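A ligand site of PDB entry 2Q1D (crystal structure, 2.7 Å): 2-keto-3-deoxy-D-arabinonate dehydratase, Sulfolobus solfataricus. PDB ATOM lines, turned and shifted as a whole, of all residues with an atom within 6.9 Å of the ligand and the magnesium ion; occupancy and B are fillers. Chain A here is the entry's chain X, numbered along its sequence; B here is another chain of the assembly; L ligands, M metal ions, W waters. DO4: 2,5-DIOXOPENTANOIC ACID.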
ATOM      1  N   GLY A  78      29.236  21.860  11.162  1.00  0.00           N
ATOM      2  CA  GLY A  78      28.092  21.667  12.048  1.00  0.00           C
ATOM      3  C   GLY A  78      26.947  20.864  11.485  1.00  0.00           C
ATOM      4  O   GLY A  78      26.689  20.870  10.271  1.00  0.00           O
ATOM      5  N   SER A  79      26.252  20.179  12.384  1.00  0.00           N
ATOM      6  CA  SER A  79      24.998  19.507  12.076  1.00  0.00           C
ATOM      7  C   SER A  79      23.812  20.285  12.676  1.00  0.00           C
ATOM      8  O   SER A  79      23.936  20.902  13.740  1.00  0.00           O
ATOM      9  CB  SER A  79      25.020  18.089  12.635  1.00  0.00           C
ATOM     10  OG  SER A  79      24.548  17.157  11.683  1.00  0.00           O
ATOM     11  N   GLY A  80      22.673  20.232  11.987  1.00  0.00           N
ATOM     12  CA  GLY A  80      21.463  20.923  12.416  1.00  0.00           C
ATOM     13  C   GLY A  80      20.249  20.032  12.631  1.00  0.00           C
ATOM     14  O   GLY A  80      20.021  19.076  11.885  1.00  0.00           O
ATOM     15  N   ILE A  81      19.483  20.362  13.674  1.00  0.00           N
ATOM     16  CA  ILE A  81      18.192  19.721  14.001  1.00  0.00           C
ATOM     17  C   ILE A  81      18.298  18.198  14.138  1.00  0.00           C
ATOM     18  O   ILE A  81      17.692  17.423  13.394  1.00  0.00           O
ATOM     19  CB  ILE A  81      17.046  20.158  13.051  1.00  0.00           C
ATOM     20  CG1 ILE A  81      16.966  21.686  12.979  1.00  0.00           C
ATOM     21  CG2 ILE A  81      15.715  19.706  13.587  1.00  0.00           C
ATOM     22  CD1 ILE A  81      17.906  22.323  11.968  1.00  0.00           C
ATOM     23  N   SER A  82      19.081  17.787  15.118  1.00  0.00           N
ATOM     24  CA  SER A  82      19.322  16.384  15.336  1.00  0.00           C
ATOM     25  C   SER A  82      18.558  15.881  16.567  1.00  0.00           C
ATOM     26  O   SER A  82      18.724  14.725  16.988  1.00  0.00           O
ATOM     27  CB  SER A  82      20.823  16.156  15.463  1.00  0.00           C
ATOM     28  OG  SER A  82      21.456  17.304  16.013  1.00  0.00           O
ATOM     29  N   TYR A  83      17.715  16.756  17.134  1.00  0.00           N
ATOM     30  CA  TYR A  83      16.863  16.439  18.287  1.00  0.00           C
ATOM     31  C   TYR A  83      15.374  16.749  17.979  1.00  0.00           C
ATOM     32  O   TYR A  83      14.446  16.345  18.705  1.00  0.00           O
ATOM     33  CB  TYR A  83      17.311  17.242  19.530  1.00  0.00           C
ATOM     34  CG  TYR A  83      18.698  16.905  20.089  1.00  0.00           C
ATOM     35  CD1 TYR A  83      19.867  17.418  19.497  1.00  0.00           C
ATOM     36  CD2 TYR A  83      18.850  16.128  21.260  1.00  0.00           C
ATOM     37  CE1 TYR A  83      21.140  17.133  20.018  1.00  0.00           C
ATOM     38  CE2 TYR A  83      20.123  15.848  21.790  1.00  0.00           C
ATOM     39  CZ  TYR A  83      21.264  16.359  21.164  1.00  0.00           C
ATOM     40  OH  TYR A  83      22.521  16.103  21.670  1.00  0.00           O
ATOM     41  N   TYR A 104      12.711  23.752   8.922  1.00  0.00           N
ATOM     42  CA  TYR A 104      13.347  23.009  10.007  1.00  0.00           C
ATOM     43  C   TYR A 104      12.674  21.670  10.261  1.00  0.00           C
ATOM     44  O   TYR A 104      13.363  20.668  10.486  1.00  0.00           O
ATOM     45  CB  TYR A 104      13.422  23.846  11.297  1.00  0.00           C
ATOM     46  CG  TYR A 104      14.213  25.118  11.122  1.00  0.00           C
ATOM     47  CD1 TYR A 104      15.589  25.128  11.300  1.00  0.00           C
ATOM     48  CD2 TYR A 104      13.581  26.300  10.750  1.00  0.00           C
ATOM     49  CE1 TYR A 104      16.321  26.293  11.117  1.00  0.00           C
ATOM     50  CE2 TYR A 104      14.303  27.465  10.567  1.00  0.00           C
ATOM     51  CZ  TYR A 104      15.668  27.458  10.752  1.00  0.00           C
ATOM     52  OH  TYR A 104      16.380  28.625  10.568  1.00  0.00           O
ATOM     53  N   GLU A 114      20.823  18.140   7.871  1.00  0.00           N
ATOM     54  CA  GLU A 114      21.508  19.410   7.638  1.00  0.00           C
ATOM     55  C   GLU A 114      22.978  19.310   8.036  1.00  0.00           C
ATOM     56  O   GLU A 114      23.319  18.745   9.093  1.00  0.00           O
ATOM     57  CB  GLU A 114      20.835  20.555   8.406  1.00  0.00           C
ATOM     58  CG  GLU A 114      21.436  21.942   8.093  1.00  0.00           C
ATOM     59  CD  GLU A 114      20.941  23.063   9.001  1.00  0.00           C
ATOM     60  OE1 GLU A 114      20.149  22.784   9.939  1.00  0.00           O
ATOM     61  OE2 GLU A 114      21.334  24.227   8.773  1.00  0.00           O
ATOM     62  N   PHE A 116      26.433  22.057   7.792  1.00  0.00           N
ATOM     63  CA  PHE A 116      26.944  23.374   7.399  1.00  0.00           C
ATOM     64  C   PHE A 116      28.410  23.557   7.786  1.00  0.00           C
ATOM     65  O   PHE A 116      28.905  22.916   8.719  1.00  0.00           O
ATOM     66  CB  PHE A 116      26.083  24.515   7.985  1.00  0.00           C
ATOM     67  CG  PHE A 116      26.070  24.557   9.498  1.00  0.00           C
ATOM     68  CD1 PHE A 116      26.992  25.334  10.186  1.00  0.00           C
ATOM     69  CD2 PHE A 116      25.151  23.798  10.225  1.00  0.00           C
ATOM     70  CE1 PHE A 116      26.985  25.349  11.591  1.00  0.00           C
ATOM     71  CE2 PHE A 116      25.134  23.805  11.610  1.00  0.00           C
ATOM     72  CZ  PHE A 116      26.045  24.574  12.302  1.00  0.00           C
ATOM     73  N   GLU A 143      25.160  27.666  21.545  1.00  0.00           N
ATOM     74  CA  GLU A 143      24.569  26.347  21.286  1.00  0.00           C
ATOM     75  C   GLU A 143      25.509  25.229  21.783  1.00  0.00           C
ATOM     76  O   GLU A 143      26.486  24.880  21.120  1.00  0.00           O
ATOM     77  CB  GLU A 143      24.237  26.180  19.796  1.00  0.00           C
ATOM     78  CG  GLU A 143      23.379  27.283  19.143  1.00  0.00           C
ATOM     79  CD  GLU A 143      22.740  26.859  17.805  1.00  0.00           C
ATOM     80  OE1 GLU A 143      21.879  27.594  17.290  1.00  0.00           O
ATOM     81  OE2 GLU A 143      23.079  25.784  17.268  1.00  0.00           O
ATOM     82  N   PRO A 144      25.217  24.683  22.974  1.00  0.00           N
ATOM     83  CA  PRO A 144      26.010  23.622  23.605  1.00  0.00           C
ATOM     84  C   PRO A 144      25.837  22.297  22.890  1.00  0.00           C
ATOM     85  O   PRO A 144      24.705  21.805  22.767  1.00  0.00           O
ATOM     86  CB  PRO A 144      25.399  23.518  24.998  1.00  0.00           C
ATOM     87  CG  PRO A 144      23.973  23.962  24.807  1.00  0.00           C
ATOM     88  CD  PRO A 144      24.059  25.072  23.799  1.00  0.00           C
ATOM     89  N   GLU A 145      26.928  21.702  22.422  1.00  0.00           N
ATOM     90  CA  GLU A 145      26.837  20.509  21.582  1.00  0.00           C
ATOM     91  C   GLU A 145      27.950  19.546  21.838  1.00  0.00           C
ATOM     92  O   GLU A 145      29.057  19.955  22.185  1.00  0.00           O
ATOM     93  CB  GLU A 145      26.866  20.917  20.115  1.00  0.00           C
ATOM     94  CG  GLU A 145      25.914  22.048  19.788  1.00  0.00           C
ATOM     95  CD  GLU A 145      25.793  22.334  18.305  1.00  0.00           C
ATOM     96  OE1 GLU A 145      25.103  23.322  17.954  1.00  0.00           O
ATOM     97  OE2 GLU A 145      26.382  21.570  17.500  1.00  0.00           O
ATOM     98  N   ASP A 164      28.663  26.170  19.454  1.00  0.00           N
ATOM     99  CA  ASP A 164      28.245  26.682  18.165  1.00  0.00           C
ATOM    100  C   ASP A 164      27.534  28.030  18.352  1.00  0.00           C
ATOM    101  O   ASP A 164      26.324  28.143  18.245  1.00  0.00           O
ATOM    102  CB  ASP A 164      27.349  25.642  17.490  1.00  0.00           C
ATOM    103  CG  ASP A 164      26.748  26.117  16.167  1.00  0.00           C
ATOM    104  OD1 ASP A 164      27.295  27.019  15.482  1.00  0.00           O
ATOM    105  OD2 ASP A 164      25.689  25.548  15.797  1.00  0.00           O
ATOM    106  N   VAL A 165      28.308  29.067  18.649  1.00  0.00           N
ATOM    107  CA  VAL A 165      27.742  30.392  18.897  1.00  0.00           C
ATOM    108  C   VAL A 165      27.047  30.856  17.620  1.00  0.00           C
ATOM    109  O   VAL A 165      27.667  30.902  16.562  1.00  0.00           O
ATOM    110  CB  VAL A 165      28.858  31.396  19.288  1.00  0.00           C
ATOM    111  CG1 VAL A 165      28.275  32.732  19.772  1.00  0.00           C
ATOM    112  CG2 VAL A 165      29.799  30.758  20.324  1.00  0.00           C
ATOM    113  N   SER A 166      25.749  31.184  17.718  1.00  0.00           N
ATOM    114  CA  SER A 166      24.935  31.529  16.536  1.00  0.00           C
ATOM    115  C   SER A 166      24.098  32.794  16.702  1.00  0.00           C
ATOM    116  O   SER A 166      23.390  32.955  17.704  1.00  0.00           O
ATOM    117  CB  SER A 166      24.015  30.364  16.160  1.00  0.00           C
ATOM    118  OG  SER A 166      24.545  29.104  16.576  1.00  0.00           O
ATOM    119  N   ARG A 168      21.198  33.938  16.066  1.00  0.00           N
ATOM    120  CA  ARG A 168      19.850  33.480  15.788  1.00  0.00           C
ATOM    121  C   ARG A 168      18.902  34.487  15.143  1.00  0.00           C
ATOM    122  O   ARG A 168      17.977  34.106  14.426  1.00  0.00           O
ATOM    123  CB  ARG A 168      19.250  32.965  17.086  1.00  0.00           C
ATOM    124  CG  ARG A 168      19.956  31.740  17.624  1.00  0.00           C
ATOM    125  CD  ARG A 168      19.781  30.544  16.684  1.00  0.00           C
ATOM    126  NE  ARG A 168      18.391  30.391  16.263  1.00  0.00           N
ATOM    127  CZ  ARG A 168      17.438  29.832  17.006  1.00  0.00           C
ATOM    128  NH1 ARG A 168      17.722  29.334  18.217  1.00  0.00           N
ATOM    129  NH2 ARG A 168      16.209  29.761  16.542  1.00  0.00           N
ATOM    130  N   GLU A 171      19.516  34.713  11.388  1.00  0.00           N
ATOM    131  CA  GLU A 171      19.032  33.492  10.768  1.00  0.00           C
ATOM    132  C   GLU A 171      17.515  33.489  10.593  1.00  0.00           C
ATOM    133  O   GLU A 171      17.003  33.139   9.523  1.00  0.00           O
ATOM    134  CB  GLU A 171      19.476  32.284  11.587  1.00  0.00           C
ATOM    135  CG  GLU A 171      18.784  30.990  11.235  1.00  0.00           C
ATOM    136  CD  GLU A 171      19.093  29.888  12.221  1.00  0.00           C
ATOM    137  OE1 GLU A 171      19.958  30.088  13.108  1.00  0.00           O
ATOM    138  OE2 GLU A 171      18.470  28.804  12.127  1.00  0.00           O
ATOM    139  N   LEU A 178      22.265  32.227   7.105  1.00  0.00           N
ATOM    140  CA  LEU A 178      22.842  31.247   8.021  1.00  0.00           C
ATOM    141  C   LEU A 178      24.382  31.313   8.102  1.00  0.00           C
ATOM    142  O   LEU A 178      24.930  31.299   9.209  1.00  0.00           O
ATOM    143  CB  LEU A 178      22.369  29.826   7.693  1.00  0.00           C
ATOM    144  CG  LEU A 178      22.623  28.773   8.797  1.00  0.00           C
ATOM    145  CD1 LEU A 178      21.584  28.940   9.916  1.00  0.00           C
ATOM    146  CD2 LEU A 178      22.646  27.316   8.259  1.00  0.00           C
ATOM    147  N   SER A 181      25.429  34.220  10.013  1.00  0.00           N
ATOM    148  CA  SER A 181      25.011  33.988  11.373  1.00  0.00           C
ATOM    149  C   SER A 181      25.925  33.013  12.101  1.00  0.00           C
ATOM    150  O   SER A 181      25.972  33.029  13.331  1.00  0.00           O
ATOM    151  CB  SER A 181      23.583  33.472  11.406  1.00  0.00           C
ATOM    152  OG  SER A 181      23.544  32.076  11.611  1.00  0.00           O
ATOM    153  N   LYS A 182      26.644  32.182  11.355  1.00  0.00           N
ATOM    154  CA  LYS A 182      27.437  31.078  11.939  1.00  0.00           C
ATOM    155  C   LYS A 182      28.972  31.246  11.950  1.00  0.00           C
ATOM    156  O   LYS A 182      29.650  30.682  12.810  1.00  0.00           O
ATOM    157  CB  LYS A 182      27.068  29.745  11.276  1.00  0.00           C
ATOM    158  CG  LYS A 182      25.673  29.193  11.624  1.00  0.00           C
ATOM    159  CD  LYS A 182      25.648  28.528  12.991  1.00  0.00           C
ATOM    160  CE  LYS A 182      24.324  27.883  13.230  1.00  0.00           C
ATOM    161  NZ  LYS A 182      24.300  27.141  14.500  1.00  0.00           N
ATOM    162  N   THR A 253      30.444  19.171  14.824  1.00  0.00           N
ATOM    163  CA  THR A 253      29.603  19.446  15.989  1.00  0.00           C
ATOM    164  C   THR A 253      28.174  18.986  15.709  1.00  0.00           C
ATOM    165  O   THR A 253      27.522  19.421  14.745  1.00  0.00           O
ATOM    166  CB  THR A 253      29.707  20.937  16.492  1.00  0.00           C
ATOM    167  OG1 THR A 253      28.841  21.130  17.618  1.00  0.00           O
ATOM    168  CG2 THR A 253      29.344  21.931  15.423  1.00  0.00           C
ATOM    169  N   THR A 254      27.687  18.100  16.565  1.00  0.00           N
ATOM    170  CA  THR A 254      26.502  17.305  16.251  1.00  0.00           C
ATOM    171  C   THR A 254      25.114  17.952  16.463  1.00  0.00           C
ATOM    172  O   THR A 254      24.115  17.235  16.439  1.00  0.00           O
ATOM    173  CB  THR A 254      26.536  15.960  16.997  1.00  0.00           C
ATOM    174  OG1 THR A 254      26.509  16.205  18.415  1.00  0.00           O
ATOM    175  CG2 THR A 254      27.805  15.194  16.638  1.00  0.00           C
ATOM    176  N   GLY A 255      25.046  19.276  16.652  1.00  0.00           N
ATOM    177  CA  GLY A 255      23.760  19.955  16.864  1.00  0.00           C
ATOM    178  C   GLY A 255      23.334  20.075  18.337  1.00  0.00           C
ATOM    179  O   GLY A 255      23.688  19.229  19.172  1.00  0.00           O
ATOM    180  N   THR A 256      22.566  21.118  18.663  1.00  0.00           N
ATOM    181  CA  THR A 256      22.183  21.412  20.046  1.00  0.00           C
ATOM    182  C   THR A 256      20.749  21.067  20.352  1.00  0.00           C
ATOM    183  O   THR A 256      19.893  21.087  19.463  1.00  0.00           O
ATOM    184  CB  THR A 256      22.388  22.901  20.400  1.00  0.00           C
ATOM    185  OG1 THR A 256      22.343  23.057  21.814  1.00  0.00           O
ATOM    186  CG2 THR A 256      21.294  23.762  19.784  1.00  0.00           C
ATOM    187  N   ALA A 257      20.483  20.781  21.633  1.00  0.00           N
ATOM    188  CA  ALA A 257      19.125  20.565  22.147  1.00  0.00           C
ATOM    189  C   ALA A 257      18.680  21.590  23.221  1.00  0.00           C
ATOM    190  O   ALA A 257      17.605  21.447  23.800  1.00  0.00           O
ATOM    191  CB  ALA A 257      18.987  19.148  22.689  1.00  0.00           C
ATOM    192  N   VAL A 259      17.899  25.558  23.934  1.00  0.00           N
ATOM    193  CA  VAL A 259      17.664  26.821  23.219  1.00  0.00           C
ATOM    194  C   VAL A 259      16.926  27.874  24.082  1.00  0.00           C
ATOM    195  O   VAL A 259      15.698  27.846  24.172  1.00  0.00           O
ATOM    196  CB  VAL A 259      16.879  26.562  21.887  1.00  0.00           C
ATOM    197  CG1 VAL A 259      16.774  27.831  21.053  1.00  0.00           C
ATOM    198  CG2 VAL A 259      17.539  25.460  21.066  1.00  0.00           C
ATOM    199  N   LEU B 176      18.442  24.761   3.700  1.00  0.00           N
ATOM    200  CA  LEU B 176      19.390  24.298   4.710  1.00  0.00           C
ATOM    201  C   LEU B 176      20.413  23.304   4.149  1.00  0.00           C
ATOM    202  O   LEU B 176      21.350  22.898   4.846  1.00  0.00           O
ATOM    203  CB  LEU B 176      18.659  23.686   5.904  1.00  0.00           C
ATOM    204  CG  LEU B 176      17.782  24.674   6.661  1.00  0.00           C
ATOM    205  CD1 LEU B 176      16.915  23.963   7.675  1.00  0.00           C
ATOM    206  CD2 LEU B 176      18.642  25.758   7.325  1.00  0.00           C
HETATM  207  O3  DO4 L   1      19.748  26.702  11.803  1.00  0.00           O
HETATM  208  C5  DO4 L   1      20.368  25.672  11.586  1.00  0.00           C
HETATM  209  C4  DO4 L   1      21.454  25.244  12.541  1.00  0.00           C
HETATM  210  C3  DO4 L   1      20.875  24.249  13.544  1.00  0.00           C
HETATM  211  C2  DO4 L   1      21.918  23.983  14.598  1.00  0.00           C
HETATM  212  O5  DO4 L   1      22.999  24.560  14.557  1.00  0.00           O
HETATM  213  C1  DO4 L   1      21.669  23.041  15.687  1.00  0.00           C
HETATM  214  O1  DO4 L   1      20.582  22.419  15.749  1.00  0.00           O
HETATM  215  O2  DO4 L   1      22.586  22.883  16.533  1.00  0.00           O
HETATM  216 MG    MG M   1      24.335  24.202  16.140  1.00  0.00          MG
HETATM  217  O   HOH W   1      25.522  22.721  15.359  1.00  0.00           O
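The backbone NH of Ile 81 sits at hydrogen-bond distance from an oxygen (O1) of the ligand. The backbone NH (N) of Thr 256 lies close to an oxygen (O2) of the ligand (2.8 Å). The side-chain carboxylate (OE2) of Glu 171 sits close to an oxygen (O3) of the ligand (2.5 Å). O5 of the ligand sits close to NZ of Lys 182 (2.9 Å).
The side-chain carboxylate (OE2) of Glu 145 sits at hydrogen-bond distance from the side-chain hydroxyl (OG1) of Thr 253. The backbone NH (N) of Thr 256 lies close to the side-chain carboxylate (OE1) of Glu 145 (3.4 Å). The side-chain carboxylate of Asp 164 lies within salt-bridge range of the side-chain amino group of Lys 182 (3.2 Å). The side-chain carboxylate (OE2) of Glu 145 is in hydrogen-bond range of the backbone NH (N) of Gly 255, 2.8 Å away. O of Glu 114 sits at hydrogen-bond distance from OG of Ser 79, 3.3 Å away. O of Thr 253 lies within hydrogen-bond range of N of Ser 79. The side-chain hydroxyl (OH) of Tyr 104 sits at hydrogen-bond distance from the side-chain carboxylate (OE2) of Glu 171 (2.6 Å). N of Gly 80 sits at hydrogen-bond distance from O of Glu 114 (3.3 Å).
Merely in contact with the ligand: Ser 79 (3.7 Å), Gly 80 (3.6 Å), Tyr 104 (3.5 Å), Glu 114 (3.3 Å), Phe 116 (3.7 Å), Leu 178 (3.5 Å) and Gly 255 (3.2 Å). Within 4 Å of the ligand: Ser 79, Gly 80, Ile 81, Tyr 104, Glu 114, Phe 116, Glu 143, Glu 145, Asp 164, Glu 171, Leu 178, Lys 182, Gly 255 and Thr 256.
Lys 182 touches the magnesium ion (NZ to MG, 3.4 Å). Four residues have an atom within 4 Å of the magnesium ion: Glu 143, Glu 145, Asp 164 and Lys 182.
The magnesium ion is bound by the side-chain carboxylate (OD2) of Asp 164 (1.9 Å), water W1 (2.1 Å), an oxygen (O5) of the ligand (2.1 Å), the side-chain carboxylate (OE1) of Glu 145 (2.2 Å), an oxygen (O2) of the ligand (2.2 Å) and the side-chain carboxylate (OE2) of Glu 143 (2.3 Å). The magnesium ion has six donor atoms within binding distance.
Water W1 lies within hydrogen-bond range of OE2 of Glu 145 (2.6 Å) and O of Ser 79 (2.9 Å).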
